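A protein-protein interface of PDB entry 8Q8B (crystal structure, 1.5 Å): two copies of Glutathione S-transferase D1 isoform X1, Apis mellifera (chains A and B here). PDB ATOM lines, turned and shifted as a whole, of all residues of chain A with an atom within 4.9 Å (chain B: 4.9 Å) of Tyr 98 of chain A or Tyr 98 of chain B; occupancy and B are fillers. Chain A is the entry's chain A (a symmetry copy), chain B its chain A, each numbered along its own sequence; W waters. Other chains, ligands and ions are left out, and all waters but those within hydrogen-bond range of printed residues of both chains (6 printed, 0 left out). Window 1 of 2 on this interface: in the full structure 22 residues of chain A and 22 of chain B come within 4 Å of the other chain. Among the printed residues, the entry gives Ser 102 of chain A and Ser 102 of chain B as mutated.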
ATOM      1  N   GLU A  64      -6.562   5.454   4.541  1.00  0.00           N
ATOM      2  CA  GLU A  64      -6.673   6.214   5.790  1.00  0.00           C
ATOM      3  C   GLU A  64      -8.050   5.955   6.390  1.00  0.00           C
ATOM      4  O   GLU A  64      -9.051   6.507   5.921  1.00  0.00           O
ATOM      5  CB  GLU A  64      -6.408   7.709   5.592  1.00  0.00           C
ATOM      6  CG  GLU A  64      -6.139   8.442   6.873  1.00  0.00           C
ATOM      7  CD  GLU A  64      -4.878   7.950   7.576  1.00  0.00           C
ATOM      8  OE1 GLU A  64      -3.826   7.754   6.916  1.00  0.00           O
ATOM      9  OE2 GLU A  64      -4.941   7.753   8.801  1.00  0.00           O
ATOM     10  N   ARG A  66      -9.862   6.761   8.947  1.00  0.00           N
ATOM     11  CA  ARG A  66     -10.800   7.779   9.404  1.00  0.00           C
ATOM     12  C   ARG A  66     -11.290   8.648   8.254  1.00  0.00           C
ATOM     13  O   ARG A  66     -12.408   9.186   8.319  1.00  0.00           O
ATOM     14  CB  ARG A  66     -10.162   8.600  10.525  1.00  0.00           C
ATOM     15  CG  ARG A  66      -9.923   7.720  11.730  1.00  0.00           C
ATOM     16  CD  ARG A  66      -8.939   8.334  12.696  1.00  0.00           C
ATOM     17  NE  ARG A  66      -8.591   7.356  13.718  1.00  0.00           N
ATOM     18  CZ  ARG A  66      -7.675   6.410  13.561  1.00  0.00           C
ATOM     19  NH1 ARG A  66      -6.970   6.309  12.445  1.00  0.00           N
ATOM     20  NH2 ARG A  66      -7.461   5.545  14.546  1.00  0.00           N
ATOM     21  N   ALA A  67     -10.497   8.772   7.179  1.00  0.00           N
ATOM     22  CA  ALA A  67     -11.004   9.440   5.979  1.00  0.00           C
ATOM     23  C   ALA A  67     -12.012   8.558   5.253  1.00  0.00           C
ATOM     24  O   ALA A  67     -12.989   9.068   4.690  1.00  0.00           O
ATOM     25  CB  ALA A  67      -9.858   9.800   5.024  1.00  0.00           C
ATOM     26  N   ASN A  94     -14.708  15.264  14.335  1.00  0.00           N
ATOM     27  CA  ASN A  94     -13.396  15.314  13.694  1.00  0.00           C
ATOM     28  C   ASN A  94     -12.295  15.420  14.730  1.00  0.00           C
ATOM     29  O   ASN A  94     -11.284  14.712  14.659  1.00  0.00           O
ATOM     30  CB  ASN A  94     -13.320  16.495  12.739  1.00  0.00           C
ATOM     31  CG  ASN A  94     -14.204  16.321  11.526  1.00  0.00           C
ATOM     32  OD1 ASN A  94     -14.553  15.204  11.157  1.00  0.00           O
ATOM     33  ND2 ASN A  94     -14.555  17.431  10.886  1.00  0.00           N
ATOM     34  N   GLN A  95     -12.483  16.301  15.708  1.00  0.00           N
ATOM     35  CA  GLN A  95     -11.509  16.440  16.779  1.00  0.00           C
ATOM     36  C   GLN A  95     -11.255  15.101  17.461  1.00  0.00           C
ATOM     37  O   GLN A  95     -10.104  14.704  17.683  1.00  0.00           O
ATOM     38  CB  GLN A  95     -12.025  17.465  17.776  1.00  0.00           C
ATOM     39  CG  GLN A  95     -11.215  17.615  19.015  1.00  0.00           C
ATOM     40  CD  GLN A  95     -11.999  18.413  20.050  1.00  0.00           C
ATOM     41  OE1 GLN A  95     -12.734  17.851  20.868  1.00  0.00           O
ATOM     42  NE2 GLN A  95     -11.892  19.726  19.976  1.00  0.00           N
ATOM     43  N   ARG A  96     -12.321  14.379  17.786  1.00  0.00           N
ATOM     44  CA  ARG A  96     -12.131  13.113  18.487  1.00  0.00           C
ATOM     45  C   ARG A  96     -11.472  12.066  17.596  1.00  0.00           C
ATOM     46  O   ARG A  96     -10.740  11.209  18.094  1.00  0.00           O
ATOM     47  CB  ARG A  96     -13.462  12.594  19.018  1.00  0.00           C
ATOM     48  CG  ARG A  96     -13.323  11.570  20.128  1.00  0.00           C
ATOM     49  CD  ARG A  96     -12.899  12.210  21.464  1.00  0.00           C
ATOM     50  NE  ARG A  96     -13.910  13.119  21.998  1.00  0.00           N
ATOM     51  CZ  ARG A  96     -13.839  14.441  21.946  1.00  0.00           C
ATOM     52  NH1 ARG A  96     -12.778  15.060  21.450  1.00  0.00           N
ATOM     53  NH2 ARG A  96     -14.856  15.164  22.407  1.00  0.00           N
ATOM     54  N   LEU A  97     -11.714  12.126  16.280  1.00  0.00           N
ATOM     55  CA  LEU A  97     -11.034  11.224  15.360  1.00  0.00           C
ATOM     56  C   LEU A  97      -9.531  11.485  15.340  1.00  0.00           C
ATOM     57  O   LEU A  97      -8.740  10.536  15.314  1.00  0.00           O
ATOM     58  CB  LEU A  97     -11.639  11.362  13.959  1.00  0.00           C
ATOM     59  CG  LEU A  97     -13.012  10.701  13.780  1.00  0.00           C
ATOM     60  CD1 LEU A  97     -13.605  11.063  12.427  1.00  0.00           C
ATOM     61  CD2 LEU A  97     -12.969   9.175  13.948  1.00  0.00           C
ATOM     62  N   TYR A  98      -9.108  12.753  15.348  1.00  0.00           N
ATOM     63  CA  TYR A  98      -7.672  13.015  15.427  1.00  0.00           C
ATOM     64  C   TYR A  98      -7.100  12.510  16.740  1.00  0.00           C
ATOM     65  O   TYR A  98      -5.994  11.966  16.771  1.00  0.00           O
ATOM     66  CB  TYR A  98      -7.361  14.503  15.264  1.00  0.00           C
ATOM     67  CG  TYR A  98      -7.637  15.080  13.894  1.00  0.00           C
ATOM     68  CD1 TYR A  98      -6.882  14.722  12.787  1.00  0.00           C
ATOM     69  CD2 TYR A  98      -8.641  16.017  13.730  1.00  0.00           C
ATOM     70  CE1 TYR A  98      -7.154  15.273  11.542  1.00  0.00           C
ATOM     71  CE2 TYR A  98      -8.914  16.573  12.506  1.00  0.00           C
ATOM     72  CZ  TYR A  98      -8.176  16.200  11.413  1.00  0.00           C
ATOM     73  OH  TYR A  98      -8.489  16.783  10.194  1.00  0.00           O
ATOM     74  N   PHE A  99      -7.839  12.689  17.841  1.00  0.00           N
ATOM     75  CA  PHE A  99      -7.388  12.169  19.130  1.00  0.00           C
ATOM     76  C   PHE A  99      -7.254  10.656  19.080  1.00  0.00           C
ATOM     77  O   PHE A  99      -6.264  10.082  19.552  1.00  0.00           O
ATOM     78  CB  PHE A  99      -8.371  12.568  20.238  1.00  0.00           C
ATOM     79  CG  PHE A  99      -8.235  11.723  21.479  1.00  0.00           C
ATOM     80  CD1 PHE A  99      -7.236  11.986  22.404  1.00  0.00           C
ATOM     81  CD2 PHE A  99      -9.074  10.641  21.698  1.00  0.00           C
ATOM     82  CE1 PHE A  99      -7.097  11.196  23.536  1.00  0.00           C
ATOM     83  CE2 PHE A  99      -8.924   9.850  22.829  1.00  0.00           C
ATOM     84  CZ  PHE A  99      -7.936  10.127  23.732  1.00  0.00           C
ATOM     85  N   ASP A 100      -8.265   9.992  18.528  1.00  0.00           N
ATOM     86  CA  ASP A 100      -8.233   8.545  18.393  1.00  0.00           C
ATOM     87  C   ASP A 100      -6.965   8.089  17.679  1.00  0.00           C
ATOM     88  O   ASP A 100      -6.284   7.159  18.124  1.00  0.00           O
ATOM     89  CB  ASP A 100      -9.490   8.090  17.644  1.00  0.00           C
ATOM     90  CG  ASP A 100      -9.488   6.615  17.351  1.00  0.00           C
ATOM     91  OD1 ASP A 100      -9.370   5.820  18.303  1.00  0.00           O
ATOM     92  OD2 ASP A 100      -9.609   6.247  16.166  1.00  0.00           O
ATOM     93  N   MET A 101      -6.631   8.739  16.561  1.00  0.00           N
ATOM     94  CA  MET A 101      -5.435   8.368  15.814  1.00  0.00           C
ATOM     95  C   MET A 101      -4.169   8.660  16.607  1.00  0.00           C
ATOM     96  O   MET A 101      -3.309   7.784  16.768  1.00  0.00           O
ATOM     97  CB  MET A 101      -5.395   9.110  14.481  1.00  0.00           C
ATOM     98  CG  MET A 101      -4.079   8.943  13.712  1.00  0.00           C
ATOM     99  SD  MET A 101      -4.211   9.649  12.061  1.00  0.00           S
ATOM    100  CE  MET A 101      -3.243  11.122  12.054  1.00  0.00           C
ATOM    101  N   SER A 102      -4.032   9.891  17.090  1.00  0.00           N
ATOM    102  CA  SER A 102      -2.743  10.386  17.561  1.00  0.00           C
ATOM    103  C   SER A 102      -2.429   9.996  18.994  1.00  0.00           C
ATOM    104  O   SER A 102      -1.250   9.974  19.370  1.00  0.00           O
ATOM    105  CB  SER A 102      -2.683  11.906  17.442  1.00  0.00           C
ATOM    106  OG  SER A 102      -3.727  12.519  18.176  1.00  0.00           O
ATOM    107  N   SER A 103      -3.448   9.703  19.796  1.00  0.00           N
ATOM    108  CA  SER A 103      -3.263   9.296  21.182  1.00  0.00           C
ATOM    109  C   SER A 103      -3.653   7.840  21.402  1.00  0.00           C
ATOM    110  O   SER A 103      -2.817   7.033  21.816  1.00  0.00           O
ATOM    111  CB  SER A 103      -4.066  10.213  22.110  1.00  0.00           C
ATOM    112  OG  SER A 103      -3.488  11.500  22.158  1.00  0.00           O
ATOM    113  N   GLU B  64      -7.611  21.350  18.363  1.00  0.00           N
ATOM    114  CA  GLU B  64      -7.153  20.455  17.296  1.00  0.00           C
ATOM    115  C   GLU B  64      -7.123  21.239  15.989  1.00  0.00           C
ATOM    116  O   GLU B  64      -8.171  21.486  15.384  1.00  0.00           O
ATOM    117  CB  GLU B  64      -8.009  19.190  17.183  1.00  0.00           C
ATOM    118  CG  GLU B  64      -7.360  18.099  16.384  1.00  0.00           C
ATOM    119  CD  GLU B  64      -6.068  17.595  17.019  1.00  0.00           C
ATOM    120  OE1 GLU B  64      -6.024  17.364  18.254  1.00  0.00           O
ATOM    121  OE2 GLU B  64      -5.086  17.434  16.277  1.00  0.00           O
ATOM    122  N   ARG B  66      -6.412  20.862  12.855  1.00  0.00           N
ATOM    123  CA  ARG B  66      -7.009  20.442  11.593  1.00  0.00           C
ATOM    124  C   ARG B  66      -8.527  20.357  11.691  1.00  0.00           C
ATOM    125  O   ARG B  66      -9.221  20.526  10.675  1.00  0.00           O
ATOM    126  CB  ARG B  66      -6.378  19.127  11.137  1.00  0.00           C
ATOM    127  CG  ARG B  66      -4.916  19.343  10.825  1.00  0.00           C
ATOM    128  CD  ARG B  66      -4.146  18.046  10.778  1.00  0.00           C
ATOM    129  NE  ARG B  66      -2.721  18.333  10.685  1.00  0.00           N
ATOM    130  CZ  ARG B  66      -1.952  18.621  11.726  1.00  0.00           C
ATOM    131  NH1 ARG B  66      -2.434  18.635  12.960  1.00  0.00           N
ATOM    132  NH2 ARG B  66      -0.669  18.902  11.526  1.00  0.00           N
ATOM    133  N   ALA B  67      -9.066  20.133  12.899  1.00  0.00           N
ATOM    134  CA  ALA B  67     -10.516  20.229  13.072  1.00  0.00           C
ATOM    135  C   ALA B  67     -10.972  21.681  13.030  1.00  0.00           C
ATOM    136  O   ALA B  67     -12.057  21.976  12.513  1.00  0.00           O
ATOM    137  CB  ALA B  67     -10.955  19.593  14.398  1.00  0.00           C
ATOM    138  N   ASN B  94      -9.046  15.276   3.545  1.00  0.00           N
ATOM    139  CA  ASN B  94      -9.017  14.704   4.889  1.00  0.00           C
ATOM    140  C   ASN B  94      -7.872  13.721   5.031  1.00  0.00           C
ATOM    141  O   ASN B  94      -7.130  13.746   6.020  1.00  0.00           O
ATOM    142  CB  ASN B  94     -10.334  14.006   5.194  1.00  0.00           C
ATOM    143  CG  ASN B  94     -11.485  14.974   5.339  1.00  0.00           C
ATOM    144  OD1 ASN B  94     -11.286  16.149   5.629  1.00  0.00           O
ATOM    145  ND2 ASN B  94     -12.703  14.476   5.157  1.00  0.00           N
ATOM    146  N   GLN B  95      -7.710  12.851   4.039  1.00  0.00           N
ATOM    147  CA  GLN B  95      -6.608  11.902   4.056  1.00  0.00           C
ATOM    148  C   GLN B  95      -5.273  12.622   4.207  1.00  0.00           C
ATOM    149  O   GLN B  95      -4.431  12.241   5.031  1.00  0.00           O
ATOM    150  CB  GLN B  95      -6.642  11.092   2.771  1.00  0.00           C
ATOM    151  CG  GLN B  95      -5.489  10.176   2.562  1.00  0.00           C
ATOM    152  CD  GLN B  95      -5.480   9.680   1.120  1.00  0.00           C
ATOM    153  OE1 GLN B  95      -4.867  10.290   0.239  1.00  0.00           O
ATOM    154  NE2 GLN B  95      -6.208   8.610   0.869  1.00  0.00           N
ATOM    155  N   ARG B  96      -5.067  13.679   3.432  1.00  0.00           N
ATOM    156  CA  ARG B  96      -3.784  14.370   3.503  1.00  0.00           C
ATOM    157  C   ARG B  96      -3.603  15.089   4.835  1.00  0.00           C
ATOM    158  O   ARG B  96      -2.473  15.221   5.312  1.00  0.00           O
ATOM    159  CB  ARG B  96      -3.645  15.354   2.348  1.00  0.00           C
ATOM    160  CG  ARG B  96      -2.214  15.766   2.061  1.00  0.00           C
ATOM    161  CD  ARG B  96      -1.412  14.648   1.368  1.00  0.00           C
ATOM    162  NE  ARG B  96      -1.921  14.332   0.036  1.00  0.00           N
ATOM    163  CZ  ARG B  96      -2.654  13.268  -0.259  1.00  0.00           C
ATOM    164  NH1 ARG B  96      -2.930  12.343   0.649  1.00  0.00           N
ATOM    165  NH2 ARG B  96      -3.118  13.122  -1.497  1.00  0.00           N
ATOM    166  N   LEU B  97      -4.699  15.552   5.449  1.00  0.00           N
ATOM    167  CA  LEU B  97      -4.610  16.153   6.772  1.00  0.00           C
ATOM    168  C   LEU B  97      -4.163  15.132   7.815  1.00  0.00           C
ATOM    169  O   LEU B  97      -3.346  15.453   8.684  1.00  0.00           O
ATOM    170  CB  LEU B  97      -5.957  16.777   7.149  1.00  0.00           C
ATOM    171  CG  LEU B  97      -6.279  18.099   6.440  1.00  0.00           C
ATOM    172  CD1 LEU B  97      -7.709  18.526   6.732  1.00  0.00           C
ATOM    173  CD2 LEU B  97      -5.304  19.228   6.806  1.00  0.00           C
ATOM    174  N   TYR B  98      -4.680  13.901   7.758  1.00  0.00           N
ATOM    175  CA  TYR B  98      -4.189  12.887   8.689  1.00  0.00           C
ATOM    176  C   TYR B  98      -2.718  12.596   8.447  1.00  0.00           C
ATOM    177  O   TYR B  98      -1.954  12.410   9.396  1.00  0.00           O
ATOM    178  CB  TYR B  98      -4.997  11.593   8.591  1.00  0.00           C
ATOM    179  CG  TYR B  98      -6.430  11.683   9.065  1.00  0.00           C
ATOM    180  CD1 TYR B  98      -6.745  11.868  10.403  1.00  0.00           C
ATOM    181  CD2 TYR B  98      -7.466  11.541   8.160  1.00  0.00           C
ATOM    182  CE1 TYR B  98      -8.070  11.941  10.811  1.00  0.00           C
ATOM    183  CE2 TYR B  98      -8.778  11.603   8.552  1.00  0.00           C
ATOM    184  CZ  TYR B  98      -9.082  11.807   9.873  1.00  0.00           C
ATOM    185  OH  TYR B  98     -10.422  11.868  10.225  1.00  0.00           O
ATOM    186  N   PHE B  99      -2.303  12.543   7.176  1.00  0.00           N
ATOM    187  CA  PHE B  99      -0.891  12.337   6.864  1.00  0.00           C
ATOM    188  C   PHE B  99      -0.047  13.469   7.426  1.00  0.00           C
ATOM    189  O   PHE B  99       1.011  13.244   8.028  1.00  0.00           O
ATOM    190  CB  PHE B  99      -0.690  12.242   5.346  1.00  0.00           C
ATOM    191  CG  PHE B  99       0.738  12.478   4.926  1.00  0.00           C
ATOM    192  CD1 PHE B  99       1.676  11.459   5.016  1.00  0.00           C
ATOM    193  CD2 PHE B  99       1.154  13.724   4.484  1.00  0.00           C
ATOM    194  CE1 PHE B  99       2.995  11.681   4.649  1.00  0.00           C
ATOM    195  CE2 PHE B  99       2.478  13.941   4.126  1.00  0.00           C
ATOM    196  CZ  PHE B  99       3.387  12.924   4.218  1.00  0.00           C
ATOM    197  N   ASP B 100      -0.496  14.701   7.213  1.00  0.00           N
ATOM    198  CA  ASP B 100       0.208  15.861   7.735  1.00  0.00           C
ATOM    199  C   ASP B 100       0.442  15.732   9.236  1.00  0.00           C
ATOM    200  O   ASP B 100       1.551  15.964   9.729  1.00  0.00           O
ATOM    201  CB  ASP B 100      -0.597  17.121   7.402  1.00  0.00           C
ATOM    202  CG  ASP B 100      -0.006  18.364   8.006  1.00  0.00           C
ATOM    203  OD1 ASP B 100       1.175  18.653   7.735  1.00  0.00           O
ATOM    204  OD2 ASP B 100      -0.725  19.059   8.751  1.00  0.00           O
ATOM    205  N   MET B 101      -0.600  15.358   9.982  1.00  0.00           N
ATOM    206  CA  MET B 101      -0.466  15.210  11.427  1.00  0.00           C
ATOM    207  C   MET B 101       0.465  14.061  11.786  1.00  0.00           C
ATOM    208  O   MET B 101       1.408  14.235  12.570  1.00  0.00           O
ATOM    209  CB  MET B 101      -1.835  14.987  12.063  1.00  0.00           C
ATOM    210  CG  MET B 101      -1.781  14.619  13.551  1.00  0.00           C
ATOM    211  SD  MET B 101      -3.433  14.609  14.266  1.00  0.00           S
ATOM    212  CE  MET B 101      -3.855  12.923  14.560  1.00  0.00           C
ATOM    213  N   SER B 102       0.203  12.879  11.237  1.00  0.00           N
ATOM    214  CA  SER B 102       0.796  11.651  11.753  1.00  0.00           C
ATOM    215  C   SER B 102       2.188  11.376  11.214  1.00  0.00           C
ATOM    216  O   SER B 102       2.950  10.641  11.856  1.00  0.00           O
ATOM    217  CB  SER B 102      -0.098  10.456  11.434  1.00  0.00           C
ATOM    218  OG  SER B 102      -0.313  10.334  10.041  1.00  0.00           O
ATOM    219  N   SER B 103       2.528  11.933  10.057  1.00  0.00           N
ATOM    220  CA  SER B 103       3.843  11.755   9.457  1.00  0.00           C
ATOM    221  C   SER B 103       4.644  13.051   9.453  1.00  0.00           C
ATOM    222  O   SER B 103       5.725  13.110  10.044  1.00  0.00           O
ATOM    223  CB  SER B 103       3.702  11.206   8.034  1.00  0.00           C
ATOM    224  OG  SER B 103       3.266   9.864   8.060  1.00  0.00           O
HETATM  225  O   HOH W   1     -11.045  14.061  11.647  1.00  0.00           O
HETATM  226  O   HOH W   2     -11.031  17.878  10.262  1.00  0.00           O
HETATM  227  O   HOH W   3      -8.893  14.991   8.233  1.00  0.00           O
HETATM  228  O   HOH W   4     -11.991  12.376   8.002  1.00  0.00           O
HETATM  229  O   HOH W   5     -14.155  20.344  11.629  1.00  0.00           O
HETATM  230  O   HOH W   6     -13.588  11.752   4.159  1.00  0.00           O
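OD2 of Asp 100 of chain B is in salt-bridge range of NH2 of Arg 66 of chain B (2.8 Å). NH1 of Arg 96 of chain B sits at hydrogen-bond distance from OE1 of Gln 95 of chain B (2.9 Å). The side-chain hydroxyl of Ser 102 of chain B is in hydrogen-bond range of the backbone carbonyl oxygen of Tyr 98 of chain B (2.7 Å). The guanidinium group (NH2) of Arg 66 of chain A lies within salt-bridge range of the side-chain carboxylate (OD2) of Asp 100 of chain A. The side-chain amide oxygen (OE1) of Gln 95 of chain A is in hydrogen-bond range of the guanidinium group (NH1) of Arg 96 of chain A. O of Tyr 98 of chain A sits at hydrogen-bond distance from OG of Ser 102 of chain A, at 2.7 Å.
Glu 64 of chain A touches Tyr 98 of chain B. Gln 95 of chain B touches Ala 67 of chain A (N to CB, 3.9 Å). CD1 of Leu 97 of chain A touches OH of Tyr 98 of chain B (3.95 Å). CB of Arg 66 of chain B touches OH of Tyr 98 of chain A, at 3.3 Å. Ala 67 of chain B touches Tyr 98 of chain A. Tyr 98 of chain A touches Leu 97 of chain B (OH to CD1, 3.95 Å). Tyr 98 of chain B touches Tyr 98 of chain A (CE1 to CE1, 3.5 Å). Met 101 of chain B touches Met 101 of chain A. Met 101 of chain A touches Ser 102 of chain B. Ser 102 of chain A touches Met 101 of chain B (CB to CE, 3.3 Å).
Glu 64 of chain A touches Tyr 98 of chain B, and with the chains exchanged Tyr 98 of chain A touches Glu 64 of chain B. Ala 67 of chain A touches Gln 95 of chain B, and with the chains exchanged Gln 95 of chain A touches Ala 67 of chain B. Leu 97 of chain A touches Tyr 98 of chain B, and with the chains exchanged Tyr 98 of chain A touches Leu 97 of chain B. Tyr 98 of chain A touches Met 101 of chain B, and with the chains exchanged Met 101 of chain A touches Tyr 98 of chain B. Positions printed for both chains: 64, 66, 67, 94, 95, 96, 97, 98, 99, 100, 101, 102 and 103. Of the 16 pairs that touch across the chains among the printed residues, 16 have their exchanged pair printed and touching as well.
Printed residues of chain B within 4 Å of Arg 66 of chain A: Tyr 98. Tyr 98 of chain A touches just these residues of chain B: Glu 64, Arg 66, Ala 67, Leu 97, Tyr 98 and Met 101. Of the printed residues of chain B, Ser 102 of chain A touches Met 101. Of the printed residues of chain A, Glu 64 of chain B touches Tyr 98. Printed residues of chain A within 4 Å of Arg 66 of chain B: Tyr 98. Tyr 98 of chain B touches six residues of chain A. Asp 100 of chain B touches none of the printed residues of chain A. Printed residues of chain A within 4 Å of Met 101 of chain B: Tyr 98, Met 101 and Ser 102. The nearest printed residue of chain B that does not touch Tyr 98 of chain A is Asn 94 of chain B (5.3 Å). The nearest printed residue of chain B that does not touch Met 101 of chain A is Phe 99 of chain B (5.2 Å).
Of the 13 printed residues of chain B, 8 touch a printed residue of chain A. Printed residues of chain B that touch a printed residue of chain A: Glu 64, Arg 66, Ala 67, Gln 95, Leu 97, Tyr 98, Met 101 and Ser 102. Hydrophobic or aromatic side chains of chain A within 4 Å of the printed part of chain B: Ala 67, Leu 97, Tyr 98 and Met 101. Among the printed residues, no Asp or Glu carboxylate lies within 4 Å of a Lys or Arg side-chain nitrogen of the other chain.
Water W1 lies within hydrogen-bond range of OH of Tyr 98 of chain B (2.7 Å) and O of Asn 94 of chain A (3.1 Å). Water W3 lies within hydrogen-bond range of the side-chain hydroxyl of Tyr 98 of chain A (2.7 Å) and the backbone carbonyl oxygen of Asn 94 of chain B (3.1 Å). Water W2 lies within hydrogen-bond range of the side-chain hydroxyl of Tyr 98 of chain A and the backbone carbonyl oxygen of Arg 66 of chain B. Water W4 bridges the side-chain hydroxyl of Tyr 98 of chain B and the backbone carbonyl oxygen of Arg 66 of chain A. Water W5 lies within hydrogen-bond range of O of Ala 67 of chain B and ND2 of Asn 94 of chain A. Water W6 bridges the backbone carbonyl oxygen of Ala 67 of chain A (2.8 Å) and the side-chain amide nitrogen of Asn 94 of chain B (3.0 Å).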
